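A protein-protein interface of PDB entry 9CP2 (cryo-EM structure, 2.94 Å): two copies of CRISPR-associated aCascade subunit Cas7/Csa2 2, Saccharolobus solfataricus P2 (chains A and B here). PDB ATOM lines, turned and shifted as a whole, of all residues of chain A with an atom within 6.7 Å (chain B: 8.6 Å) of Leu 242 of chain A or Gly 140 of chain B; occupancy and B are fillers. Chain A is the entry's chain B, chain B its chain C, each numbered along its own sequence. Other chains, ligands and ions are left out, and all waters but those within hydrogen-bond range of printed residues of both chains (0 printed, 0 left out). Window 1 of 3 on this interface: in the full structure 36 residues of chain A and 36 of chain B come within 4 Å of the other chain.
Of the 26 printed residues of chain B, 11 touch a printed residue of chain A. Hydrophobic or aromatic side chains of chain B that line the printed part of chain A: Ala 54, Tyr 141, Ile 143, Met 260 and Pro 263. Of the 11 printed residues of chain A, 7 touch a printed residue of chain B. Hydrophobic or aromatic side chains of chain A within 4 Å of the printed part of chain B: Leu 12, Phe 241 and Leu 242. Among the printed residues, 16 pairs touch across the chains. Among the printed residues, no Asp or Glu carboxylate lies within 4 Å of a Lys or Arg side-chain nitrogen of the other chain.
The guanidinium group (NH2) of Arg 238 of chain A is in hydrogen-bond range of the side-chain sulfur (SD) of Met 260 of chain B (3.6 Å). The backbone NH (N) of Leu 139 of chain B sits at hydrogen-bond distance from the backbone carbonyl oxygen (O) of Ser 239 of chain A, 2.6 Å away. The backbone NH (N) of Leu 242 of chain A is in hydrogen-bond range of the backbone carbonyl oxygen (O) of Leu 139 of chain B (3.3 Å). The backbone carbonyl oxygen of Arg 240 of chain A sits close to the backbone carbonyl oxygen of Leu 139 of chain B. The guanidinium group of Arg 240 of chain A is in hydrogen-bond range of the backbone carbonyl oxygen of Ile 137 of chain B (3.5 Å).
No position is printed for both chains. Of the 16 pairs that touch across the chains among the printed residues, none has its exchanged pair printed and touching as well.
Leu 242 of chain A touches just these residues of chain B: Leu 139 (3.3 Å), Gly 140 (3.9 Å) and Ser 187 (3.97 Å). Gly 140 of chain B touches just one residue of chain A: Leu 242. No residue of chain B comes within 4 Å of Pro 243 of chain A. Printed residues of chain B within 4 Å of Arg 240 of chain A: Gly 50, Ala 54, Ile 137 and Leu 139. Printed residues of chain A within 4 Å of Leu 139 of chain B: Ser 239, Arg 240, Phe 241 and Leu 242. Printed residues of chain B within 4 Å of Arg 238 of chain A: Lys 138 and Met 260. Printed residues of chain A within 4 Å of Tyr 141 of chain B: Leu 12 and Phe 241. Ile 48 of chain B touches none of the printed residues of chain A. Phe 188 of chain B touches none of the printed residues of chain A.
N of Thr 185 of chain B sits at hydrogen-bond distance from O of Ile 143 of chain B, 3.0 Å away. N of Lys 138 of chain B sits at hydrogen-bond distance from O of Glu 189 of chain B (3.0 Å).
Among the printed residues, merely in contact across the chains: Ser 239 of chain A with Lys 138 of chain B (3.3 Å), Phe 241 of chain A with Tyr 141 of chain B (3.3 Å), Leu 12 of chain A with Ile 143 of chain B (3.5 Å), Arg 240 of chain A with Ala 54 of chain B (3.5 Å), Leu 12 of chain A with Tyr 141 of chain B (3.5 Å), Phe 241 of chain A with Leu 139 of chain B (3.7 Å), Ser 244 of chain A with Pro 263 of chain B (3.7 Å), Arg 238 of chain A with Lys 138 of chain B (3.8 Å), Leu 242 of chain A with Gly 140 of chain B (3.9 Å), Arg 240 of chain A with Gly 50 of chain B (3.9 Å) and Leu 242 of chain A with Ser 187 of chain B (3.97 Å).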
ATOM      1  N   ASN A  11     -25.750  28.915 -16.015  1.00  0.00           N
ATOM      2  CA  ASN A  11     -25.950  29.387 -17.378  1.00  0.00           C
ATOM      3  C   ASN A  11     -25.204  28.504 -18.367  1.00  0.00           C
ATOM      4  O   ASN A  11     -24.090  28.052 -18.092  1.00  0.00           O
ATOM      5  CB  ASN A  11     -25.477  30.831 -17.540  1.00  0.00           C
ATOM      6  CG  ASN A  11     -26.152  31.771 -16.578  1.00  0.00           C
ATOM      7  OD1 ASN A  11     -25.531  32.696 -16.060  1.00  0.00           O
ATOM      8  ND2 ASN A  11     -27.433  31.547 -16.334  1.00  0.00           N
ATOM      9  N   LEU A  12     -25.825  28.279 -19.524  1.00  0.00           N
ATOM     10  CA  LEU A  12     -25.230  27.556 -20.649  1.00  0.00           C
ATOM     11  C   LEU A  12     -24.675  26.204 -20.195  1.00  0.00           C
ATOM     12  O   LEU A  12     -23.475  25.939 -20.214  1.00  0.00           O
ATOM     13  CB  LEU A  12     -24.157  28.402 -21.336  1.00  0.00           C
ATOM     14  CG  LEU A  12     -24.706  29.351 -22.402  1.00  0.00           C
ATOM     15  CD1 LEU A  12     -25.393  30.548 -21.768  1.00  0.00           C
ATOM     16  CD2 LEU A  12     -23.618  29.793 -23.355  1.00  0.00           C
ATOM     17  N   GLU A  13     -25.606  25.353 -19.787  1.00  0.00           N
ATOM     18  CA  GLU A  13     -25.293  24.124 -19.080  1.00  0.00           C
ATOM     19  C   GLU A  13     -25.973  22.935 -19.737  1.00  0.00           C
ATOM     20  O   GLU A  13     -27.084  23.051 -20.262  1.00  0.00           O
ATOM     21  CB  GLU A  13     -25.735  24.246 -17.618  1.00  0.00           C
ATOM     22  CG  GLU A  13     -25.790  22.952 -16.843  1.00  0.00           C
ATOM     23  CD  GLU A  13     -27.143  22.279 -16.943  1.00  0.00           C
ATOM     24  OE1 GLU A  13     -28.160  22.997 -17.028  1.00  0.00           O
ATOM     25  OE2 GLU A  13     -27.190  21.032 -16.952  1.00  0.00           O
ATOM     26  N   LYS A 237     -20.415  16.079 -19.198  1.00  0.00           N
ATOM     27  CA  LYS A 237     -20.073  16.934 -20.334  1.00  0.00           C
ATOM     28  C   LYS A 237     -19.366  18.208 -19.883  1.00  0.00           C
ATOM     29  O   LYS A 237     -19.646  19.302 -20.372  1.00  0.00           O
ATOM     30  CB  LYS A 237     -21.313  17.266 -21.165  1.00  0.00           C
ATOM     31  CG  LYS A 237     -21.799  16.106 -22.010  1.00  0.00           C
ATOM     32  CD  LYS A 237     -22.711  16.567 -23.123  1.00  0.00           C
ATOM     33  CE  LYS A 237     -23.292  15.382 -23.864  1.00  0.00           C
ATOM     34  NZ  LYS A 237     -23.531  15.705 -25.294  1.00  0.00           N
ATOM     35  N   ARG A 238     -18.441  18.067 -18.939  1.00  0.00           N
ATOM     36  CA  ARG A 238     -17.721  19.211 -18.400  1.00  0.00           C
ATOM     37  C   ARG A 238     -16.513  19.612 -19.232  1.00  0.00           C
ATOM     38  O   ARG A 238     -15.950  20.684 -18.993  1.00  0.00           O
ATOM     39  CB  ARG A 238     -17.269  18.922 -16.965  1.00  0.00           C
ATOM     40  CG  ARG A 238     -18.395  18.900 -15.950  1.00  0.00           C
ATOM     41  CD  ARG A 238     -17.927  18.328 -14.625  1.00  0.00           C
ATOM     42  NE  ARG A 238     -17.091  19.270 -13.893  1.00  0.00           N
ATOM     43  CZ  ARG A 238     -17.547  20.320 -13.224  1.00  0.00           C
ATOM     44  NH1 ARG A 238     -18.840  20.596 -13.170  1.00  0.00           N
ATOM     45  NH2 ARG A 238     -16.686  21.110 -12.591  1.00  0.00           N
ATOM     46  N   SER A 239     -16.102  18.790 -20.201  1.00  0.00           N
ATOM     47  CA  SER A 239     -14.877  19.081 -20.940  1.00  0.00           C
ATOM     48  C   SER A 239     -15.052  20.272 -21.876  1.00  0.00           C
ATOM     49  O   SER A 239     -14.202  21.169 -21.912  1.00  0.00           O
ATOM     50  CB  SER A 239     -14.432  17.844 -21.717  1.00  0.00           C
ATOM     51  OG  SER A 239     -15.483  17.343 -22.522  1.00  0.00           O
ATOM     52  N   ARG A 240     -16.141  20.304 -22.638  1.00  0.00           N
ATOM     53  CA  ARG A 240     -16.405  21.407 -23.550  1.00  0.00           C
ATOM     54  C   ARG A 240     -17.632  22.221 -23.176  1.00  0.00           C
ATOM     55  O   ARG A 240     -17.841  23.292 -23.756  1.00  0.00           O
ATOM     56  CB  ARG A 240     -16.570  20.884 -24.984  1.00  0.00           C
ATOM     57  CG  ARG A 240     -15.541  19.841 -25.378  1.00  0.00           C
ATOM     58  CD  ARG A 240     -14.380  20.457 -26.142  1.00  0.00           C
ATOM     59  NE  ARG A 240     -13.258  19.534 -26.256  1.00  0.00           N
ATOM     60  CZ  ARG A 240     -12.157  19.605 -25.521  1.00  0.00           C
ATOM     61  NH1 ARG A 240     -11.979  20.570 -24.636  1.00  0.00           N
ATOM     62  NH2 ARG A 240     -11.210  18.687 -25.682  1.00  0.00           N
ATOM     63  N   PHE A 241     -18.442  21.750 -22.230  1.00  0.00           N
ATOM     64  CA  PHE A 241     -19.637  22.458 -21.796  1.00  0.00           C
ATOM     65  C   PHE A 241     -19.528  22.782 -20.314  1.00  0.00           C
ATOM     66  O   PHE A 241     -20.464  22.536 -19.548  1.00  0.00           O
ATOM     67  CB  PHE A 241     -20.895  21.632 -22.073  1.00  0.00           C
ATOM     68  CG  PHE A 241     -21.178  21.429 -23.533  1.00  0.00           C
ATOM     69  CD1 PHE A 241     -21.643  22.470 -24.313  1.00  0.00           C
ATOM     70  CD2 PHE A 241     -20.982  20.193 -24.124  1.00  0.00           C
ATOM     71  CE1 PHE A 241     -21.900  22.288 -25.656  1.00  0.00           C
ATOM     72  CE2 PHE A 241     -21.240  20.005 -25.467  1.00  0.00           C
ATOM     73  CZ  PHE A 241     -21.700  21.054 -26.233  1.00  0.00           C
ATOM     74  N   LEU A 242     -18.381  23.306 -19.903  1.00  0.00           N
ATOM     75  CA  LEU A 242     -18.161  23.644 -18.503  1.00  0.00           C
ATOM     76  C   LEU A 242     -19.127  24.741 -18.084  1.00  0.00           C
ATOM     77  O   LEU A 242     -19.127  25.819 -18.693  1.00  0.00           O
ATOM     78  CB  LEU A 242     -16.717  24.092 -18.294  1.00  0.00           C
ATOM     79  CG  LEU A 242     -16.200  24.137 -16.858  1.00  0.00           C
ATOM     80  CD1 LEU A 242     -15.873  22.738 -16.368  1.00  0.00           C
ATOM     81  CD2 LEU A 242     -14.983  25.038 -16.756  1.00  0.00           C
ATOM     82  N   PRO A 243     -19.958  24.523 -17.071  1.00  0.00           N
ATOM     83  CA  PRO A 243     -20.958  25.526 -16.700  1.00  0.00           C
ATOM     84  C   PRO A 243     -20.351  26.665 -15.902  1.00  0.00           C
ATOM     85  O   PRO A 243     -19.228  26.591 -15.403  1.00  0.00           O
ATOM     86  CB  PRO A 243     -21.949  24.730 -15.847  1.00  0.00           C
ATOM     87  CG  PRO A 243     -21.123  23.652 -15.249  1.00  0.00           C
ATOM     88  CD  PRO A 243     -20.075  23.297 -16.265  1.00  0.00           C
ATOM     89  N   SER A 244     -21.129  27.735 -15.786  1.00  0.00           N
ATOM     90  CA  SER A 244     -20.743  28.925 -15.033  1.00  0.00           C
ATOM     91  C   SER A 244     -21.639  29.003 -13.799  1.00  0.00           C
ATOM     92  O   SER A 244     -22.671  29.674 -13.804  1.00  0.00           O
ATOM     93  CB  SER A 244     -20.862  30.172 -15.901  1.00  0.00           C
ATOM     94  OG  SER A 244     -20.617  31.341 -15.146  1.00  0.00           O
ATOM     95  N   SER B   3      -5.627  26.046 -12.972  1.00  0.00           N
ATOM     96  CA  SER B   3      -6.931  26.590 -13.314  1.00  0.00           C
ATOM     97  C   SER B   3      -6.801  28.079 -13.588  1.00  0.00           C
ATOM     98  O   SER B   3      -5.801  28.705 -13.238  1.00  0.00           O
ATOM     99  CB  SER B   3      -7.945  26.347 -12.192  1.00  0.00           C
ATOM    100  OG  SER B   3      -8.176  24.962 -12.003  1.00  0.00           O
ATOM    101  N   GLY B   4      -7.817  28.648 -14.221  1.00  0.00           N
ATOM    102  CA  GLY B   4      -7.761  30.069 -14.502  1.00  0.00           C
ATOM    103  C   GLY B   4      -9.074  30.619 -15.002  1.00  0.00           C
ATOM    104  O   GLY B   4      -9.956  29.881 -15.451  1.00  0.00           O
ATOM    105  N   SER B   5      -9.180  31.943 -14.921  1.00  0.00           N
ATOM    106  CA  SER B   5     -10.293  32.702 -15.471  1.00  0.00           C
ATOM    107  C   SER B   5      -9.747  33.891 -16.244  1.00  0.00           C
ATOM    108  O   SER B   5      -8.752  34.505 -15.836  1.00  0.00           O
ATOM    109  CB  SER B   5     -11.244  33.180 -14.375  1.00  0.00           C
ATOM    110  OG  SER B   5     -11.854  32.080 -13.724  1.00  0.00           O
ATOM    111  N   ILE B  48     -20.015  32.450 -28.093  1.00  0.00           N
ATOM    112  CA  ILE B  48     -19.049  31.716 -28.902  1.00  0.00           C
ATOM    113  C   ILE B  48     -18.852  30.352 -28.261  1.00  0.00           C
ATOM    114  O   ILE B  48     -18.585  30.263 -27.058  1.00  0.00           O
ATOM    115  CB  ILE B  48     -17.709  32.466 -29.016  1.00  0.00           C
ATOM    116  CG1 ILE B  48     -17.881  33.738 -29.842  1.00  0.00           C
ATOM    117  CG2 ILE B  48     -16.654  31.573 -29.635  1.00  0.00           C
ATOM    118  CD1 ILE B  48     -16.767  34.732 -29.658  1.00  0.00           C
ATOM    119  N   SER B  49     -18.980  29.297 -29.058  1.00  0.00           N
ATOM    120  CA  SER B  49     -19.006  27.954 -28.500  1.00  0.00           C
ATOM    121  C   SER B  49     -17.647  27.569 -27.928  1.00  0.00           C
ATOM    122  O   SER B  49     -16.654  28.287 -28.064  1.00  0.00           O
ATOM    123  CB  SER B  49     -19.423  26.935 -29.556  1.00  0.00           C
ATOM    124  OG  SER B  49     -18.309  26.506 -30.315  1.00  0.00           O
ATOM    125  N   GLY B  50     -17.619  26.412 -27.275  1.00  0.00           N
ATOM    126  CA  GLY B  50     -16.439  25.871 -26.644  1.00  0.00           C
ATOM    127  C   GLY B  50     -15.668  24.857 -27.449  1.00  0.00           C
ATOM    128  O   GLY B  50     -14.718  24.265 -26.931  1.00  0.00           O
ATOM    129  N   GLU B  51     -16.048  24.621 -28.705  1.00  0.00           N
ATOM    130  CA  GLU B  51     -15.329  23.643 -29.511  1.00  0.00           C
ATOM    131  C   GLU B  51     -14.404  24.300 -30.524  1.00  0.00           C
ATOM    132  O   GLU B  51     -13.500  23.640 -31.046  1.00  0.00           O
ATOM    133  CB  GLU B  51     -16.317  22.709 -30.204  1.00  0.00           C
ATOM    134  CG  GLU B  51     -17.236  22.002 -29.229  1.00  0.00           C
ATOM    135  CD  GLU B  51     -17.652  20.632 -29.709  1.00  0.00           C
ATOM    136  OE1 GLU B  51     -17.368  20.302 -30.875  1.00  0.00           O
ATOM    137  OE2 GLU B  51     -18.255  19.880 -28.915  1.00  0.00           O
ATOM    138  N   ALA B  52     -14.605  25.585 -30.820  1.00  0.00           N
ATOM    139  CA  ALA B  52     -13.595  26.325 -31.567  1.00  0.00           C
ATOM    140  C   ALA B  52     -12.314  26.465 -30.755  1.00  0.00           C
ATOM    141  O   ALA B  52     -11.205  26.314 -31.286  1.00  0.00           O
ATOM    142  CB  ALA B  52     -14.135  27.697 -31.966  1.00  0.00           C
ATOM    143  N   LEU B  53     -12.454  26.746 -29.457  1.00  0.00           N
ATOM    144  CA  LEU B  53     -11.293  26.894 -28.588  1.00  0.00           C
ATOM    145  C   LEU B  53     -10.503  25.596 -28.499  1.00  0.00           C
ATOM    146  O   LEU B  53      -9.267  25.606 -28.556  1.00  0.00           O
ATOM    147  CB  LEU B  53     -11.743  27.344 -27.200  1.00  0.00           C
ATOM    148  CG  LEU B  53     -12.731  28.509 -27.174  1.00  0.00           C
ATOM    149  CD1 LEU B  53     -13.145  28.835 -25.750  1.00  0.00           C
ATOM    150  CD2 LEU B  53     -12.134  29.723 -27.848  1.00  0.00           C
ATOM    151  N   ALA B  54     -11.201  24.468 -28.358  1.00  0.00           N
ATOM    152  CA  ALA B  54     -10.521  23.180 -28.306  1.00  0.00           C
ATOM    153  C   ALA B  54      -9.785  22.891 -29.608  1.00  0.00           C
ATOM    154  O   ALA B  54      -8.666  22.367 -29.593  1.00  0.00           O
ATOM    155  CB  ALA B  54     -11.525  22.070 -27.999  1.00  0.00           C
ATOM    156  N   ILE B 137      -7.854  18.893 -20.722  1.00  0.00           N
ATOM    157  CA  ILE B 137      -8.144  20.320 -20.698  1.00  0.00           C
ATOM    158  C   ILE B 137      -9.650  20.492 -20.819  1.00  0.00           C
ATOM    159  O   ILE B 137     -10.284  19.867 -21.678  1.00  0.00           O
ATOM    160  CB  ILE B 137      -7.408  21.076 -21.819  1.00  0.00           C
ATOM    161  CG1 ILE B 137      -7.923  22.512 -21.922  1.00  0.00           C
ATOM    162  CG2 ILE B 137      -7.539  20.346 -23.144  1.00  0.00           C
ATOM    163  CD1 ILE B 137      -7.087  23.399 -22.802  1.00  0.00           C
ATOM    164  N   LYS B 138     -10.223  21.321 -19.949  1.00  0.00           N
ATOM    165  CA  LYS B 138     -11.660  21.545 -19.906  1.00  0.00           C
ATOM    166  C   LYS B 138     -11.949  23.011 -20.184  1.00  0.00           C
ATOM    167  O   LYS B 138     -11.354  23.895 -19.561  1.00  0.00           O
ATOM    168  CB  LYS B 138     -12.232  21.121 -18.553  1.00  0.00           C
ATOM    169  CG  LYS B 138     -11.614  19.841 -18.027  1.00  0.00           C
ATOM    170  CD  LYS B 138     -12.600  19.019 -17.221  1.00  0.00           C
ATOM    171  CE  LYS B 138     -12.105  17.591 -17.062  1.00  0.00           C
ATOM    172  NZ  LYS B 138     -13.126  16.711 -16.434  1.00  0.00           N
ATOM    173  N   LEU B 139     -12.859  23.263 -21.120  1.00  0.00           N
ATOM    174  CA  LEU B 139     -13.193  24.610 -21.550  1.00  0.00           C
ATOM    175  C   LEU B 139     -14.702  24.801 -21.514  1.00  0.00           C
ATOM    176  O   LEU B 139     -15.472  23.840 -21.457  1.00  0.00           O
ATOM    177  CB  LEU B 139     -12.666  24.892 -22.961  1.00  0.00           C
ATOM    178  CG  LEU B 139     -11.154  25.053 -23.093  1.00  0.00           C
ATOM    179  CD1 LEU B 139     -10.688  24.624 -24.468  1.00  0.00           C
ATOM    180  CD2 LEU B 139     -10.758  26.490 -22.822  1.00  0.00           C
ATOM    181  N   GLY B 140     -15.118  26.069 -21.554  1.00  0.00           N
ATOM    182  CA  GLY B 140     -16.523  26.414 -21.532  1.00  0.00           C
ATOM    183  C   GLY B 140     -16.845  27.464 -22.577  1.00  0.00           C
ATOM    184  O   GLY B 140     -15.955  27.996 -23.244  1.00  0.00           O
ATOM    185  N   TYR B 141     -18.137  27.752 -22.703  1.00  0.00           N
ATOM    186  CA  TYR B 141     -18.602  28.742 -23.662  1.00  0.00           C
ATOM    187  C   TYR B 141     -18.033  30.114 -23.334  1.00  0.00           C
ATOM    188  O   TYR B 141     -17.602  30.384 -22.211  1.00  0.00           O
ATOM    189  CB  TYR B 141     -20.125  28.821 -23.659  1.00  0.00           C
ATOM    190  CG  TYR B 141     -20.819  27.887 -24.622  1.00  0.00           C
ATOM    191  CD1 TYR B 141     -20.869  26.524 -24.380  1.00  0.00           C
ATOM    192  CD2 TYR B 141     -21.441  28.372 -25.762  1.00  0.00           C
ATOM    193  CE1 TYR B 141     -21.508  25.672 -25.253  1.00  0.00           C
ATOM    194  CE2 TYR B 141     -22.084  27.525 -26.641  1.00  0.00           C
ATOM    195  CZ  TYR B 141     -22.113  26.175 -26.379  1.00  0.00           C
ATOM    196  OH  TYR B 141     -22.749  25.320 -27.247  1.00  0.00           O
ATOM    197  N   MET B 142     -18.038  30.989 -24.330  1.00  0.00           N
ATOM    198  CA  MET B 142     -17.615  32.370 -24.142  1.00  0.00           C
ATOM    199  C   MET B 142     -18.862  33.240 -24.024  1.00  0.00           C
ATOM    200  O   MET B 142     -19.469  33.608 -25.034  1.00  0.00           O
ATOM    201  CB  MET B 142     -16.722  32.819 -25.292  1.00  0.00           C
ATOM    202  CG  MET B 142     -15.545  33.656 -24.851  1.00  0.00           C
ATOM    203  SD  MET B 142     -14.551  34.233 -26.229  1.00  0.00           S
ATOM    204  CE  MET B 142     -13.491  32.815 -26.455  1.00  0.00           C
ATOM    205  N   ILE B 143     -19.237  33.568 -22.793  1.00  0.00           N
ATOM    206  CA  ILE B 143     -20.446  34.337 -22.516  1.00  0.00           C
ATOM    207  C   ILE B 143     -20.041  35.755 -22.137  1.00  0.00           C
ATOM    208  O   ILE B 143     -19.009  35.940 -21.475  1.00  0.00           O
ATOM    209  CB  ILE B 143     -21.269  33.678 -21.397  1.00  0.00           C
ATOM    210  CG1 ILE B 143     -21.637  32.249 -21.781  1.00  0.00           C
ATOM    211  CG2 ILE B 143     -22.521  34.476 -21.086  1.00  0.00           C
ATOM    212  CD1 ILE B 143     -21.704  31.309 -20.607  1.00  0.00           C
ATOM    213  N   THR B 185     -16.022  36.398 -21.302  1.00  0.00           N
ATOM    214  CA  THR B 185     -15.347  35.839 -20.139  1.00  0.00           C
ATOM    215  C   THR B 185     -15.379  34.325 -20.236  1.00  0.00           C
ATOM    216  O   THR B 185     -16.386  33.751 -20.658  1.00  0.00           O
ATOM    217  CB  THR B 185     -16.015  36.267 -18.824  1.00  0.00           C
ATOM    218  OG1 THR B 185     -17.235  35.537 -18.649  1.00  0.00           O
ATOM    219  CG2 THR B 185     -16.319  37.756 -18.817  1.00  0.00           C
ATOM    220  N   PHE B 186     -14.284  33.675 -19.846  1.00  0.00           N
ATOM    221  CA  PHE B 186     -14.305  32.218 -19.809  1.00  0.00           C
ATOM    222  C   PHE B 186     -13.231  31.701 -18.867  1.00  0.00           C
ATOM    223  O   PHE B 186     -12.223  32.366 -18.624  1.00  0.00           O
ATOM    224  CB  PHE B 186     -14.127  31.611 -21.206  1.00  0.00           C
ATOM    225  CG  PHE B 186     -12.703  31.571 -21.678  1.00  0.00           C
ATOM    226  CD1 PHE B 186     -12.037  32.736 -22.016  1.00  0.00           C
ATOM    227  CD2 PHE B 186     -12.036  30.365 -21.794  1.00  0.00           C
ATOM    228  CE1 PHE B 186     -10.731  32.697 -22.456  1.00  0.00           C
ATOM    229  CE2 PHE B 186     -10.730  30.321 -22.231  1.00  0.00           C
ATOM    230  CZ  PHE B 186     -10.077  31.489 -22.562  1.00  0.00           C
ATOM    231  N   SER B 187     -13.458  30.498 -18.351  1.00  0.00           N
ATOM    232  CA  SER B 187     -12.547  29.849 -17.425  1.00  0.00           C
ATOM    233  C   SER B 187     -12.062  28.530 -18.010  1.00  0.00           C
ATOM    234  O   SER B 187     -12.705  27.937 -18.879  1.00  0.00           O
ATOM    235  CB  SER B 187     -13.217  29.607 -16.067  1.00  0.00           C
ATOM    236  OG  SER B 187     -14.452  28.931 -16.222  1.00  0.00           O
ATOM    237  N   PHE B 188     -10.916  28.071 -17.514  1.00  0.00           N
ATOM    238  CA  PHE B 188     -10.297  26.863 -18.032  1.00  0.00           C
ATOM    239  C   PHE B 188      -9.586  26.127 -16.909  1.00  0.00           C
ATOM    240  O   PHE B 188      -9.307  26.688 -15.844  1.00  0.00           O
ATOM    241  CB  PHE B 188      -9.314  27.172 -19.166  1.00  0.00           C
ATOM    242  CG  PHE B 188      -7.997  27.710 -18.694  1.00  0.00           C
ATOM    243  CD1 PHE B 188      -7.843  29.058 -18.430  1.00  0.00           C
ATOM    244  CD2 PHE B 188      -6.913  26.869 -18.514  1.00  0.00           C
ATOM    245  CE1 PHE B 188      -6.635  29.559 -17.997  1.00  0.00           C
ATOM    246  CE2 PHE B 188      -5.704  27.365 -18.077  1.00  0.00           C
ATOM    247  CZ  PHE B 188      -5.564  28.711 -17.819  1.00  0.00           C
ATOM    248  N   GLU B 189      -9.271  24.862 -17.181  1.00  0.00           N
ATOM    249  CA  GLU B 189      -8.701  23.954 -16.198  1.00  0.00           C
ATOM    250  C   GLU B 189      -7.870  22.903 -16.921  1.00  0.00           C
ATOM    251  O   GLU B 189      -8.310  22.347 -17.929  1.00  0.00           O
ATOM    252  CB  GLU B 189      -9.806  23.287 -15.374  1.00  0.00           C
ATOM    253  CG  GLU B 189      -9.425  21.957 -14.765  1.00  0.00           C
ATOM    254  CD  GLU B 189     -10.465  21.456 -13.788  1.00  0.00           C
ATOM    255  OE1 GLU B 189     -10.957  22.266 -12.975  1.00  0.00           O
ATOM    256  OE2 GLU B 189     -10.797  20.253 -13.837  1.00  0.00           O
ATOM    257  N   LEU B 229      -4.597  29.923 -26.803  1.00  0.00           N
ATOM    258  CA  LEU B 229      -5.892  30.317 -26.260  1.00  0.00           C
ATOM    259  C   LEU B 229      -5.795  31.628 -25.491  1.00  0.00           C
ATOM    260  O   LEU B 229      -6.668  32.492 -25.618  1.00  0.00           O
ATOM    261  CB  LEU B 229      -6.448  29.210 -25.368  1.00  0.00           C
ATOM    262  CG  LEU B 229      -6.931  27.962 -26.103  1.00  0.00           C
ATOM    263  CD1 LEU B 229      -7.610  27.005 -25.142  1.00  0.00           C
ATOM    264  CD2 LEU B 229      -7.865  28.344 -27.231  1.00  0.00           C
ATOM    265  N   MET B 260     -11.643  25.632  -8.207  1.00  0.00           N
ATOM    266  CA  MET B 260     -12.193  26.371  -9.332  1.00  0.00           C
ATOM    267  C   MET B 260     -12.345  27.831  -8.925  1.00  0.00           C
ATOM    268  O   MET B 260     -13.011  28.124  -7.916  1.00  0.00           O
ATOM    269  CB  MET B 260     -13.543  25.805  -9.776  1.00  0.00           C
ATOM    270  CG  MET B 260     -13.454  24.513 -10.563  1.00  0.00           C
ATOM    271  SD  MET B 260     -15.077  23.956 -11.109  1.00  0.00           S
ATOM    272  CE  MET B 260     -15.933  23.845  -9.541  1.00  0.00           C
ATOM    273  N   PRO B 261     -11.763  28.761  -9.672  1.00  0.00           N
ATOM    274  CA  PRO B 261     -11.913  30.179  -9.341  1.00  0.00           C
ATOM    275  C   PRO B 261     -13.296  30.698  -9.701  1.00  0.00           C
ATOM    276  O   PRO B 261     -14.085  30.042 -10.381  1.00  0.00           O
ATOM    277  CB  PRO B 261     -10.832  30.857 -10.188  1.00  0.00           C
ATOM    278  CG  PRO B 261     -10.607  29.935 -11.323  1.00  0.00           C
ATOM    279  CD  PRO B 261     -10.885  28.544 -10.833  1.00  0.00           C
ATOM    280  N   PRO B 263     -16.079  32.734 -11.612  1.00  0.00           N
ATOM    281  CA  PRO B 263     -16.242  33.216 -12.987  1.00  0.00           C
ATOM    282  C   PRO B 263     -16.141  34.731 -13.045  1.00  0.00           C
ATOM    283  O   PRO B 263     -16.442  35.433 -12.078  1.00  0.00           O
ATOM    284  CB  PRO B 263     -17.644  32.735 -13.369  1.00  0.00           C
ATOM    285  CG  PRO B 263     -17.888  31.562 -12.483  1.00  0.00           C
ATOM    286  CD  PRO B 263     -17.206  31.887 -11.188  1.00  0.00           C
